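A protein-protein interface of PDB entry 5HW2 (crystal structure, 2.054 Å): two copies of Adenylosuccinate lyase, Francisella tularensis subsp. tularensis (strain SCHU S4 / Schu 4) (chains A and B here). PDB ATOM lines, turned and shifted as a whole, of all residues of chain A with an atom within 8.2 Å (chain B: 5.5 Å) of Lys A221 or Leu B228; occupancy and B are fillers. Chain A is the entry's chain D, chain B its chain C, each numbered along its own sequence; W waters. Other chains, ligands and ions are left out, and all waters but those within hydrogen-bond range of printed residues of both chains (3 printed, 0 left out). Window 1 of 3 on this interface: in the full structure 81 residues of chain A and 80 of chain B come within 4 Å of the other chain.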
ATOM      1  N   ASP A 167       8.271   6.743 -29.321  1.00  0.00           N
ATOM      2  CA  ASP A 167       8.976   7.895 -28.768  1.00  0.00           C
ATOM      3  C   ASP A 167      10.412   7.540 -28.402  1.00  0.00           C
ATOM      4  O   ASP A 167      11.341   8.297 -28.703  1.00  0.00           O
ATOM      5  CB  ASP A 167       8.228   8.434 -27.548  1.00  0.00           C
ATOM      6  CG  ASP A 167       6.908   9.088 -27.913  1.00  0.00           C
ATOM      7  OD1 ASP A 167       6.780   9.581 -29.054  1.00  0.00           O
ATOM      8  OD2 ASP A 167       5.999   9.113 -27.058  1.00  0.00           O
ATOM      9  N   LEU A 168      10.613   6.390 -27.755  1.00  0.00           N
ATOM     10  CA  LEU A 168      11.962   5.989 -27.367  1.00  0.00           C
ATOM     11  C   LEU A 168      12.804   5.619 -28.581  1.00  0.00           C
ATOM     12  O   LEU A 168      13.966   6.030 -28.685  1.00  0.00           O
ATOM     13  CB  LEU A 168      11.899   4.824 -26.382  1.00  0.00           C
ATOM     14  CG  LEU A 168      11.322   5.150 -25.006  1.00  0.00           C
ATOM     15  CD1 LEU A 168      11.274   3.903 -24.140  1.00  0.00           C
ATOM     16  CD2 LEU A 168      12.141   6.241 -24.335  1.00  0.00           C
ATOM     17  N   ASP A 170      12.520   6.641 -31.585  1.00  0.00           N
ATOM     18  CA  ASP A 170      12.887   7.852 -32.313  1.00  0.00           C
ATOM     19  C   ASP A 170      14.068   8.550 -31.652  1.00  0.00           C
ATOM     20  O   ASP A 170      14.967   9.047 -32.340  1.00  0.00           O
ATOM     21  CB  ASP A 170      11.691   8.799 -32.407  1.00  0.00           C
ATOM     22  CG  ASP A 170      10.706   8.392 -33.483  1.00  0.00           C
ATOM     23  OD1 ASP A 170      10.711   7.208 -33.879  1.00  0.00           O
ATOM     24  OD2 ASP A 170       9.924   9.258 -33.931  1.00  0.00           O
ATOM     25  N   PHE A 171      14.082   8.594 -30.318  1.00  0.00           N
ATOM     26  CA  PHE A 171      15.192   9.219 -29.608  1.00  0.00           C
ATOM     27  C   PHE A 171      16.476   8.418 -29.787  1.00  0.00           C
ATOM     28  O   PHE A 171      17.565   8.996 -29.899  1.00  0.00           O
ATOM     29  CB  PHE A 171      14.847   9.365 -28.126  1.00  0.00           C
ATOM     30  CG  PHE A 171      15.796  10.244 -27.361  1.00  0.00           C
ATOM     31  CD1 PHE A 171      16.967   9.730 -26.831  1.00  0.00           C
ATOM     32  CD2 PHE A 171      15.514  11.585 -27.168  1.00  0.00           C
ATOM     33  CE1 PHE A 171      17.840  10.537 -26.127  1.00  0.00           C
ATOM     34  CE2 PHE A 171      16.383  12.398 -26.464  1.00  0.00           C
ATOM     35  CZ  PHE A 171      17.547  11.872 -25.942  1.00  0.00           C
ATOM     36  N   ASP A 174      18.466   9.510 -32.685  1.00  0.00           N
ATOM     37  CA  ASP A 174      18.710  10.938 -32.852  1.00  0.00           C
ATOM     38  C   ASP A 174      19.312  11.594 -31.614  1.00  0.00           C
ATOM     39  O   ASP A 174      20.409  12.157 -31.677  1.00  0.00           O
ATOM     40  CB  ASP A 174      17.400  11.640 -33.228  1.00  0.00           C
ATOM     41  CG  ASP A 174      17.621  12.994 -33.882  1.00  0.00           C
ATOM     42  OD1 ASP A 174      18.607  13.681 -33.545  1.00  0.00           O
ATOM     43  OD2 ASP A 174      16.795  13.375 -34.740  1.00  0.00           O
ATOM     44  N   GLY A 175      18.602  11.521 -30.486  1.00  0.00           N
ATOM     45  CA  GLY A 175      18.871  12.401 -29.359  1.00  0.00           C
ATOM     46  C   GLY A 175      20.251  12.274 -28.745  1.00  0.00           C
ATOM     47  O   GLY A 175      20.724  13.225 -28.115  1.00  0.00           O
ATOM     48  N   PRO A 215      24.474  20.159 -24.084  1.00  0.00           N
ATOM     49  CA  PRO A 215      23.234  20.837 -23.681  1.00  0.00           C
ATOM     50  C   PRO A 215      22.266  19.870 -23.014  1.00  0.00           C
ATOM     51  O   PRO A 215      22.008  18.773 -23.513  1.00  0.00           O
ATOM     52  CB  PRO A 215      22.680  21.382 -25.006  1.00  0.00           C
ATOM     53  CG  PRO A 215      23.393  20.612 -26.076  1.00  0.00           C
ATOM     54  CD  PRO A 215      24.748  20.325 -25.520  1.00  0.00           C
ATOM     55  N   ARG A 216      21.731  20.292 -21.871  1.00  0.00           N
ATOM     56  CA  ARG A 216      20.961  19.411 -21.004  1.00  0.00           C
ATOM     57  C   ARG A 216      19.530  19.184 -21.474  1.00  0.00           C
ATOM     58  O   ARG A 216      18.824  18.375 -20.865  1.00  0.00           O
ATOM     59  CB  ARG A 216      20.951  19.964 -19.577  1.00  0.00           C
ATOM     60  CG  ARG A 216      22.128  19.493 -18.743  1.00  0.00           C
ATOM     61  CD  ARG A 216      22.133  17.980 -18.658  1.00  0.00           C
ATOM     62  NE  ARG A 216      23.328  17.457 -18.005  1.00  0.00           N
ATOM     63  CZ  ARG A 216      24.423  17.068 -18.649  1.00  0.00           C
ATOM     64  NH1 ARG A 216      25.463  16.599 -17.973  1.00  0.00           N
ATOM     65  NH2 ARG A 216      24.479  17.147 -19.972  1.00  0.00           N
ATOM     66  N   ASP A 217      19.080  19.862 -22.531  1.00  0.00           N
ATOM     67  CA  ASP A 217      17.725  19.628 -23.013  1.00  0.00           C
ATOM     68  C   ASP A 217      17.575  18.263 -23.672  1.00  0.00           C
ATOM     69  O   ASP A 217      16.451  17.765 -23.789  1.00  0.00           O
ATOM     70  CB  ASP A 217      17.307  20.732 -23.987  1.00  0.00           C
ATOM     71  CG  ASP A 217      18.147  20.750 -25.246  1.00  0.00           C
ATOM     72  OD1 ASP A 217      17.780  20.052 -26.214  1.00  0.00           O
ATOM     73  OD2 ASP A 217      19.169  21.467 -25.270  1.00  0.00           O
ATOM     74  N   ARG A 218      18.679  17.648 -24.098  1.00  0.00           N
ATOM     75  CA  ARG A 218      18.596  16.331 -24.720  1.00  0.00           C
ATOM     76  C   ARG A 218      18.225  15.264 -23.697  1.00  0.00           C
ATOM     77  O   ARG A 218      17.358  14.421 -23.951  1.00  0.00           O
ATOM     78  CB  ARG A 218      19.918  15.994 -25.408  1.00  0.00           C
ATOM     79  CG  ARG A 218      20.230  16.887 -26.596  1.00  0.00           C
ATOM     80  CD  ARG A 218      21.493  16.440 -27.307  1.00  0.00           C
ATOM     81  NE  ARG A 218      21.763  17.243 -28.495  1.00  0.00           N
ATOM     82  CZ  ARG A 218      21.349  16.930 -29.718  1.00  0.00           C
ATOM     83  NH1 ARG A 218      20.644  15.825 -29.919  1.00  0.00           N
ATOM     84  NH2 ARG A 218      21.642  17.721 -30.742  1.00  0.00           N
ATOM     85  N   ILE A 219      18.879  15.282 -22.533  1.00  0.00           N
ATOM     86  CA  ILE A 219      18.475  14.396 -21.445  1.00  0.00           C
ATOM     87  C   ILE A 219      17.066  14.741 -20.982  1.00  0.00           C
ATOM     88  O   ILE A 219      16.256  13.853 -20.686  1.00  0.00           O
ATOM     89  CB  ILE A 219      19.490  14.472 -20.288  1.00  0.00           C
ATOM     90  CG1 ILE A 219      20.703  13.589 -20.582  1.00  0.00           C
ATOM     91  CG2 ILE A 219      18.848  14.069 -18.971  1.00  0.00           C
ATOM     92  CD1 ILE A 219      21.768  13.647 -19.512  1.00  0.00           C
ATOM     93  N   ALA A 220      16.747  16.037 -20.932  1.00  0.00           N
ATOM     94  CA  ALA A 220      15.424  16.462 -20.488  1.00  0.00           C
ATOM     95  C   ALA A 220      14.325  15.875 -21.364  1.00  0.00           C
ATOM     96  O   ALA A 220      13.272  15.469 -20.859  1.00  0.00           O
ATOM     97  CB  ALA A 220      15.342  17.989 -20.474  1.00  0.00           C
ATOM     98  N   LYS A 221      14.555  15.819 -22.677  1.00  0.00           N
ATOM     99  CA  LYS A 221      13.555  15.255 -23.578  1.00  0.00           C
ATOM    100  C   LYS A 221      13.284  13.791 -23.252  1.00  0.00           C
ATOM    101  O   LYS A 221      12.127  13.355 -23.244  1.00  0.00           O
ATOM    102  CB  LYS A 221      14.012  15.402 -25.030  1.00  0.00           C
ATOM    103  CG  LYS A 221      13.033  14.835 -26.045  1.00  0.00           C
ATOM    104  CD  LYS A 221      13.537  15.011 -27.467  1.00  0.00           C
ATOM    105  CE  LYS A 221      12.509  14.530 -28.479  1.00  0.00           C
ATOM    106  NZ  LYS A 221      12.995  14.659 -29.881  1.00  0.00           N
ATOM    107  N   LEU A 222      14.336  13.022 -22.970  1.00  0.00           N
ATOM    108  CA  LEU A 222      14.152  11.606 -22.677  1.00  0.00           C
ATOM    109  C   LEU A 222      13.403  11.405 -21.365  1.00  0.00           C
ATOM    110  O   LEU A 222      12.501  10.564 -21.282  1.00  0.00           O
ATOM    111  CB  LEU A 222      15.506  10.899 -22.638  1.00  0.00           C
ATOM    112  CG  LEU A 222      15.446   9.374 -22.552  1.00  0.00           C
ATOM    113  CD1 LEU A 222      14.743   8.799 -23.769  1.00  0.00           C
ATOM    114  CD2 LEU A 222      16.843   8.796 -22.412  1.00  0.00           C
ATOM    115  N   ILE A 223      13.760  12.172 -20.333  1.00  0.00           N
ATOM    116  CA  ILE A 223      13.092  12.039 -19.040  1.00  0.00           C
ATOM    117  C   ILE A 223      11.638  12.482 -19.133  1.00  0.00           C
ATOM    118  O   ILE A 223      10.770  11.941 -18.437  1.00  0.00           O
ATOM    119  CB  ILE A 223      13.867  12.828 -17.969  1.00  0.00           C
ATOM    120  CG1 ILE A 223      15.309  12.329 -17.898  1.00  0.00           C
ATOM    121  CG2 ILE A 223      13.198  12.699 -16.611  1.00  0.00           C
ATOM    122  CD1 ILE A 223      15.421  10.858 -17.565  1.00  0.00           C
ATOM    123  N   SER A 224      11.341  13.459 -19.994  1.00  0.00           N
ATOM    124  CA  SER A 224       9.951  13.843 -20.210  1.00  0.00           C
ATOM    125  C   SER A 224       9.165  12.727 -20.888  1.00  0.00           C
ATOM    126  O   SER A 224       7.952  12.615 -20.685  1.00  0.00           O
ATOM    127  CB  SER A 224       9.877  15.126 -21.039  1.00  0.00           C
ATOM    128  OG  SER A 224      10.411  16.227 -20.324  1.00  0.00           O
ATOM    129  N   ILE A 225       9.836  11.899 -21.693  1.00  0.00           N
ATOM    130  CA  ILE A 225       9.171  10.750 -22.299  1.00  0.00           C
ATOM    131  C   ILE A 225       8.806   9.726 -21.234  1.00  0.00           C
ATOM    132  O   ILE A 225       7.699   9.175 -21.237  1.00  0.00           O
ATOM    133  CB  ILE A 225      10.061  10.134 -23.394  1.00  0.00           C
ATOM    134  CG1 ILE A 225      10.255  11.122 -24.545  1.00  0.00           C
ATOM    135  CG2 ILE A 225       9.459   8.831 -23.900  1.00  0.00           C
ATOM    136  CD1 ILE A 225      11.196  10.626 -25.622  1.00  0.00           C
ATOM    137  N   HIS A 226       9.728   9.456 -20.305  1.00  0.00           N
ATOM    138  CA  HIS A 226       9.439   8.513 -19.230  1.00  0.00           C
ATOM    139  C   HIS A 226       8.295   8.997 -18.348  1.00  0.00           C
ATOM    140  O   HIS A 226       7.610   8.184 -17.719  1.00  0.00           O
ATOM    141  CB  HIS A 226      10.697   8.268 -18.395  1.00  0.00           C
ATOM    142  CG  HIS A 226      11.705   7.391 -19.070  1.00  0.00           C
ATOM    143  ND1 HIS A 226      12.905   7.048 -18.485  1.00  0.00           N
ATOM    144  CD2 HIS A 226      11.689   6.782 -20.279  1.00  0.00           C
ATOM    145  CE1 HIS A 226      13.585   6.267 -19.305  1.00  0.00           C
ATOM    146  NE2 HIS A 226      12.870   6.090 -20.402  1.00  0.00           N
ATOM    147  N   GLY A 227       8.074  10.312 -18.287  1.00  0.00           N
ATOM    148  CA  GLY A 227       6.899  10.816 -17.597  1.00  0.00           C
ATOM    149  C   GLY A 227       5.610  10.410 -18.287  1.00  0.00           C
ATOM    150  O   GLY A 227       4.612  10.104 -17.631  1.00  0.00           O
ATOM    151  N   LEU A 228       5.616  10.400 -19.622  1.00  0.00           N
ATOM    152  CA  LEU A 228       4.448   9.941 -20.366  1.00  0.00           C
ATOM    153  C   LEU A 228       4.200   8.457 -20.136  1.00  0.00           C
ATOM    154  O   LEU A 228       3.051   8.032 -19.971  1.00  0.00           O
ATOM    155  CB  LEU A 228       4.628  10.229 -21.856  1.00  0.00           C
ATOM    156  CG  LEU A 228       5.062  11.637 -22.266  1.00  0.00           C
ATOM    157  CD1 LEU A 228       5.253  11.717 -23.773  1.00  0.00           C
ATOM    158  CD2 LEU A 228       4.051  12.666 -21.799  1.00  0.00           C
ATOM    159  N   VAL A 288      10.830  14.773 -14.166  1.00  0.00           N
ATOM    160  CA  VAL A 288      10.681  15.605 -15.357  1.00  0.00           C
ATOM    161  C   VAL A 288      11.151  17.029 -15.080  1.00  0.00           C
ATOM    162  O   VAL A 288      11.993  17.571 -15.806  1.00  0.00           O
ATOM    163  CB  VAL A 288       9.226  15.574 -15.855  1.00  0.00           C
ATOM    164  CG1 VAL A 288       9.083  16.409 -17.119  1.00  0.00           C
ATOM    165  CG2 VAL A 288       8.785  14.139 -16.108  1.00  0.00           C
ATOM    166  N   ALA A 291      14.861  17.359 -14.759  1.00  0.00           N
ATOM    167  CA  ALA A 291      15.531  17.439 -16.050  1.00  0.00           C
ATOM    168  C   ALA A 291      15.397  18.830 -16.653  1.00  0.00           C
ATOM    169  O   ALA A 291      16.337  19.336 -17.276  1.00  0.00           O
ATOM    170  CB  ALA A 291      14.964  16.381 -16.994  1.00  0.00           C
ATOM    171  N   LEU A 292      14.240  19.470 -16.466  1.00  0.00           N
ATOM    172  CA  LEU A 292      14.043  20.809 -17.012  1.00  0.00           C
ATOM    173  C   LEU A 292      14.919  21.831 -16.298  1.00  0.00           C
ATOM    174  O   LEU A 292      15.514  22.703 -16.943  1.00  0.00           O
ATOM    175  CB  LEU A 292      12.568  21.207 -16.921  1.00  0.00           C
ATOM    176  CG  LEU A 292      11.591  20.412 -17.792  1.00  0.00           C
ATOM    177  CD1 LEU A 292      10.167  20.923 -17.635  1.00  0.00           C
ATOM    178  CD2 LEU A 292      12.015  20.467 -19.245  1.00  0.00           C
ATOM    179  N   CYS A 295      18.559  22.160 -17.269  1.00  0.00           N
ATOM    180  CA  CYS A 295      18.854  22.802 -18.543  1.00  0.00           C
ATOM    181  C   CYS A 295      19.317  24.244 -18.384  1.00  0.00           C
ATOM    182  O   CYS A 295      19.890  24.800 -19.328  1.00  0.00           O
ATOM    183  CB  CYS A 295      17.621  22.771 -19.452  1.00  0.00           C
ATOM    184  SG  CYS A 295      16.970  21.124 -19.792  1.00  0.00           S
ATOM    185  N   TYR A 312      18.937  11.061  -9.912  1.00  0.00           N
ATOM    186  CA  TYR A 312      17.709  10.683 -10.601  1.00  0.00           C
ATOM    187  C   TYR A 312      17.951   9.882 -11.874  1.00  0.00           C
ATOM    188  O   TYR A 312      17.051   9.154 -12.302  1.00  0.00           O
ATOM    189  CB  TYR A 312      16.872  11.927 -10.916  1.00  0.00           C
ATOM    190  CG  TYR A 312      17.124  12.540 -12.275  1.00  0.00           C
ATOM    191  CD1 TYR A 312      18.155  13.448 -12.470  1.00  0.00           C
ATOM    192  CD2 TYR A 312      16.314  12.229 -13.360  1.00  0.00           C
ATOM    193  CE1 TYR A 312      18.383  14.015 -13.707  1.00  0.00           C
ATOM    194  CE2 TYR A 312      16.537  12.789 -14.600  1.00  0.00           C
ATOM    195  CZ  TYR A 312      17.571  13.681 -14.768  1.00  0.00           C
ATOM    196  OH  TYR A 312      17.794  14.245 -15.999  1.00  0.00           O
ATOM    197  N   GLU B 160      18.945  24.709 -30.425  1.00  0.00           N
ATOM    198  CA  GLU B 160      18.045  24.192 -29.399  1.00  0.00           C
ATOM    199  C   GLU B 160      16.590  24.421 -29.787  1.00  0.00           C
ATOM    200  O   GLU B 160      15.770  23.495 -29.745  1.00  0.00           O
ATOM    201  CB  GLU B 160      18.354  24.840 -28.050  1.00  0.00           C
ATOM    202  CG  GLU B 160      17.515  24.300 -26.902  1.00  0.00           C
ATOM    203  CD  GLU B 160      17.841  24.956 -25.573  1.00  0.00           C
ATOM    204  OE1 GLU B 160      18.528  26.000 -25.575  1.00  0.00           O
ATOM    205  OE2 GLU B 160      17.410  24.428 -24.525  1.00  0.00           O
ATOM    206  N   ARG B 164      13.381  21.667 -30.849  1.00  0.00           N
ATOM    207  CA  ARG B 164      11.974  21.701 -30.470  1.00  0.00           C
ATOM    208  C   ARG B 164      11.083  22.022 -31.661  1.00  0.00           C
ATOM    209  O   ARG B 164       9.919  21.608 -31.691  1.00  0.00           O
ATOM    210  CB  ARG B 164      11.759  22.726 -29.359  1.00  0.00           C
ATOM    211  CG  ARG B 164      12.815  22.696 -28.263  1.00  0.00           C
ATOM    212  CD  ARG B 164      12.607  21.546 -27.285  1.00  0.00           C
ATOM    213  NE  ARG B 164      13.020  20.250 -27.817  1.00  0.00           N
ATOM    214  CZ  ARG B 164      14.268  19.794 -27.799  1.00  0.00           C
ATOM    215  NH1 ARG B 164      15.241  20.529 -27.281  1.00  0.00           N
ATOM    216  NH2 ARG B 164      14.547  18.601 -28.306  1.00  0.00           N
ATOM    217  N   ASP B 167      10.471  18.738 -33.382  1.00  0.00           N
ATOM    218  CA  ASP B 167       9.564  17.963 -32.540  1.00  0.00           C
ATOM    219  C   ASP B 167       8.128  18.450 -32.690  1.00  0.00           C
ATOM    220  O   ASP B 167       7.193  17.642 -32.741  1.00  0.00           O
ATOM    221  CB  ASP B 167      10.005  18.036 -31.077  1.00  0.00           C
ATOM    222  CG  ASP B 167      11.299  17.287 -30.816  1.00  0.00           C
ATOM    223  OD1 ASP B 167      11.567  16.295 -31.527  1.00  0.00           O
ATOM    224  OD2 ASP B 167      12.045  17.687 -29.895  1.00  0.00           O
ATOM    225  N   ILE B 223       2.321  19.332 -24.603  1.00  0.00           N
ATOM    226  CA  ILE B 223       2.746  20.112 -23.444  1.00  0.00           C
ATOM    227  C   ILE B 223       4.179  19.767 -23.064  1.00  0.00           C
ATOM    228  O   ILE B 223       4.930  20.628 -22.588  1.00  0.00           O
ATOM    229  CB  ILE B 223       1.773  19.886 -22.269  1.00  0.00           C
ATOM    230  CG1 ILE B 223       0.345  20.250 -22.678  1.00  0.00           C
ATOM    231  CG2 ILE B 223       2.190  20.698 -21.058  1.00  0.00           C
ATOM    232  CD1 ILE B 223       0.146  21.720 -22.961  1.00  0.00           C
ATOM    233  N   SER B 224       4.590  18.514 -23.283  1.00  0.00           N
ATOM    234  CA  SER B 224       5.974  18.127 -23.034  1.00  0.00           C
ATOM    235  C   SER B 224       6.924  18.878 -23.958  1.00  0.00           C
ATOM    236  O   SER B 224       7.948  19.409 -23.513  1.00  0.00           O
ATOM    237  CB  SER B 224       6.138  16.616 -23.207  1.00  0.00           C
ATOM    238  OG  SER B 224       5.345  15.903 -22.277  1.00  0.00           O
ATOM    239  N   ILE B 225       6.602  18.924 -25.254  1.00  0.00           N
ATOM    240  CA  ILE B 225       7.405  19.709 -26.187  1.00  0.00           C
ATOM    241  C   ILE B 225       7.398  21.176 -25.785  1.00  0.00           C
ATOM    242  O   ILE B 225       8.396  21.884 -25.965  1.00  0.00           O
ATOM    243  CB  ILE B 225       6.901  19.520 -27.631  1.00  0.00           C
ATOM    244  CG1 ILE B 225       6.762  18.033 -27.960  1.00  0.00           C
ATOM    245  CG2 ILE B 225       7.846  20.188 -28.616  1.00  0.00           C
ATOM    246  CD1 ILE B 225       6.218  17.761 -29.349  1.00  0.00           C
ATOM    247  N   HIS B 226       6.284  21.653 -25.229  1.00  0.00           N
ATOM    248  CA  HIS B 226       6.226  23.018 -24.725  1.00  0.00           C
ATOM    249  C   HIS B 226       6.935  23.159 -23.386  1.00  0.00           C
ATOM    250  O   HIS B 226       7.434  24.243 -23.064  1.00  0.00           O
ATOM    251  CB  HIS B 226       4.770  23.471 -24.606  1.00  0.00           C
ATOM    252  CG  HIS B 226       4.085  23.634 -25.928  1.00  0.00           C
ATOM    253  ND1 HIS B 226       2.754  23.973 -26.040  1.00  0.00           N
ATOM    254  CD2 HIS B 226       4.550  23.507 -27.193  1.00  0.00           C
ATOM    255  CE1 HIS B 226       2.428  24.045 -27.319  1.00  0.00           C
ATOM    256  NE2 HIS B 226       3.499  23.767 -28.039  1.00  0.00           N
ATOM    257  N   GLY B 227       6.987  22.086 -22.594  1.00  0.00           N
ATOM    258  CA  GLY B 227       7.768  22.127 -21.370  1.00  0.00           C
ATOM    259  C   GLY B 227       9.250  22.303 -21.638  1.00  0.00           C
ATOM    260  O   GLY B 227       9.929  23.066 -20.948  1.00  0.00           O
ATOM    261  N   LEU B 228       9.768  21.602 -22.650  1.00  0.00           N
ATOM    262  CA  LEU B 228      11.171  21.768 -23.021  1.00  0.00           C
ATOM    263  C   LEU B 228      11.438  23.167 -23.556  1.00  0.00           C
ATOM    264  O   LEU B 228      12.481  23.761 -23.260  1.00  0.00           O
ATOM    265  CB  LEU B 228      11.569  20.716 -24.054  1.00  0.00           C
ATOM    266  CG  LEU B 228      11.482  19.245 -23.644  1.00  0.00           C
ATOM    267  CD1 LEU B 228      11.816  18.345 -24.821  1.00  0.00           C
ATOM    268  CD2 LEU B 228      12.411  18.964 -22.479  1.00  0.00           C
ATOM    269  N   ILE B 229      10.509  23.709 -24.350  1.00  0.00           N
ATOM    270  CA  ILE B 229      10.663  25.066 -24.873  1.00  0.00           C
ATOM    271  C   ILE B 229      10.794  26.064 -23.731  1.00  0.00           C
ATOM    272  O   ILE B 229      11.577  27.020 -23.808  1.00  0.00           O
ATOM    273  CB  ILE B 229       9.486  25.416 -25.803  1.00  0.00           C
ATOM    274  CG1 ILE B 229       9.568  24.609 -27.101  1.00  0.00           C
ATOM    275  CG2 ILE B 229       9.459  26.908 -26.105  1.00  0.00           C
ATOM    276  CD1 ILE B 229       8.398  24.832 -28.033  1.00  0.00           C
ATOM    277  N   ALA B 230      10.035  25.858 -22.652  1.00  0.00           N
ATOM    278  CA  ALA B 230      10.167  26.713 -21.476  1.00  0.00           C
ATOM    279  C   ALA B 230      11.602  26.734 -20.969  1.00  0.00           C
ATOM    280  O   ALA B 230      12.104  27.783 -20.550  1.00  0.00           O
ATOM    281  CB  ALA B 230       9.216  26.243 -20.375  1.00  0.00           C
ATOM    282  N   SER B 231      12.282  25.586 -21.006  1.00  0.00           N
ATOM    283  CA  SER B 231      13.684  25.542 -20.602  1.00  0.00           C
ATOM    284  C   SER B 231      14.570  26.286 -21.595  1.00  0.00           C
ATOM    285  O   SER B 231      15.494  27.001 -21.193  1.00  0.00           O
ATOM    286  CB  SER B 231      14.144  24.093 -20.455  1.00  0.00           C
ATOM    287  OG  SER B 231      13.378  23.409 -19.479  1.00  0.00           O
ATOM    288  N   ALA B 232      14.309  26.125 -22.895  1.00  0.00           N
ATOM    289  CA  ALA B 232      15.096  26.833 -23.899  1.00  0.00           C
ATOM    290  C   ALA B 232      14.917  28.341 -23.777  1.00  0.00           C
ATOM    291  O   ALA B 232      15.888  29.101 -23.871  1.00  0.00           O
ATOM    292  CB  ALA B 232      14.711  26.361 -25.301  1.00  0.00           C
ATOM    293  N   ILE B 233      13.679  28.790 -23.561  1.00  0.00           N
ATOM    294  CA  ILE B 233      13.423  30.215 -23.375  1.00  0.00           C
ATOM    295  C   ILE B 233      14.123  30.723 -22.121  1.00  0.00           C
ATOM    296  O   ILE B 233      14.654  31.841 -22.099  1.00  0.00           O
ATOM    297  CB  ILE B 233      11.906  30.476 -23.327  1.00  0.00           C
ATOM    298  CG1 ILE B 233      11.272  30.160 -24.683  1.00  0.00           C
ATOM    299  CG2 ILE B 233      11.611  31.909 -22.908  1.00  0.00           C
ATOM    300  CD1 ILE B 233       9.783  30.417 -24.735  1.00  0.00           C
HETATM  301  O   HOH W   1      19.816  22.842 -22.876  1.00  0.00           O
HETATM  302  O   HOH W   2      16.698  17.877 -27.486  1.00  0.00           O
HETATM  303  O   HOH W   3      18.077  24.751 -22.174  1.00  0.00           O
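Of the printed residues of chain B, Lys A221 touches Arg B164, Asp B167 and Leu B228.
Of the printed residues of chain A, Leu B228 touches Ala A220, Lys A221 and Leu A292.
Of the printed residues of chain A, Ser B231 touches Leu A292 (3.3 Å) and Cys A295 (3.9 Å).
Printed residues of chain B within 4 Å of Leu A228: Ser B224.
Of the printed residues of chain A, Glu B160 touches Asp A217 (3.5 Å).
The nearest printed residue of chain A that does not touch Leu B228 is Ser A224 (4.02 Å).
The nearest printed residue of chain B that does not touch Leu A228 is Ile B223 (7.2 Å).
The guanidinium group (NH1) of Arg B164 is in salt-bridge range of the side-chain carboxylate (OD1) of Asp A217 (2.8 Å).
The side-chain carboxylate (OD1) of Asp B167 lies within salt-bridge range of the side-chain amino group (NZ) of Lys A221 (2.7 Å).
The side-chain hydroxyl (OG) of Ser B231 sits close to the backbone carbonyl oxygen (O) of Leu A292, at 3.4 Å.
Water W2 lies within hydrogen-bond range of NH2 of Arg B164 and OD1 of Asp A217.
Water W3 bridges OE2 of Glu B160 (2.5 Å) and O of Cys A295 (3.4 Å).
Water W1 lies within hydrogen-bond range of the side-chain carboxylate (OD2) of Asp A217 (2.8 Å), the side-chain carboxylate (OE2) of Glu B160 (3.3 Å) and the backbone NH (N) of Arg A216 (3.3 Å).
Printed residues of chain A that touch a printed residue of chain B: Asp A217, Ala A220, Lys A221, Leu A228, Leu A292 and Cys A295.
Hydrophobic or aromatic side chains of chain A that line the printed part of chain B: Ala A220, Leu A228 and Leu A292.
Along chain A the printed residues that touch a printed residue of chain B span positions 217 to 295.
Hydrophobic or aromatic side chains of chain B that line the printed part of chain A: Leu B228.
Among the printed residues, 11 pairs touch across the chains.
Among the printed residues, Asp or Glu carboxylates within 4 Å of a Lys or Arg side-chain nitrogen of the other chain: Asp A217 with Arg B164 (2.8 Å) and Lys A221 with Asp B167 (2.7 Å).
Among the printed residues, merely in contact across the chains: Leu A228 with Ser B224, Asp A217 with Glu B160, Leu A292 with Leu B228, Lys A221 with Leu B228, Ala A220 with Leu B228, Leu A292 with Gly B227, Lys A221 with Arg B164 and Cys A295 with Ser B231.
Leu A228 touches Ser B224, but with the chains exchanged Ser A224 does not touch Leu B228 (4.02 Å).
Of the 11 pairs that touch across the chains among the printed residues, none has its exchanged pair printed and touching as well.
OD2 of Asp B167 lies within salt-bridge range of NH2 of Arg B164, at 3.1 Å.
SG of Cys A295 is in hydrogen-bond range of O of Arg A216 (3.5 Å).
N of Asp A217 lies close to SG of Cys A295, 3.7 Å away.
O of Ala A220 is in hydrogen-bond range of OG of Ser A224, at 3.0 Å.
The backbone carbonyl oxygen (O) of Ala A291 lies within hydrogen-bond range of the side-chain sulfur (SG) of Cys A295, at 3.2 Å.
The backbone carbonyl oxygen (O) of Leu A292 lies close to the side-chain sulfur (SG) of Cys A295 (3.6 Å).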
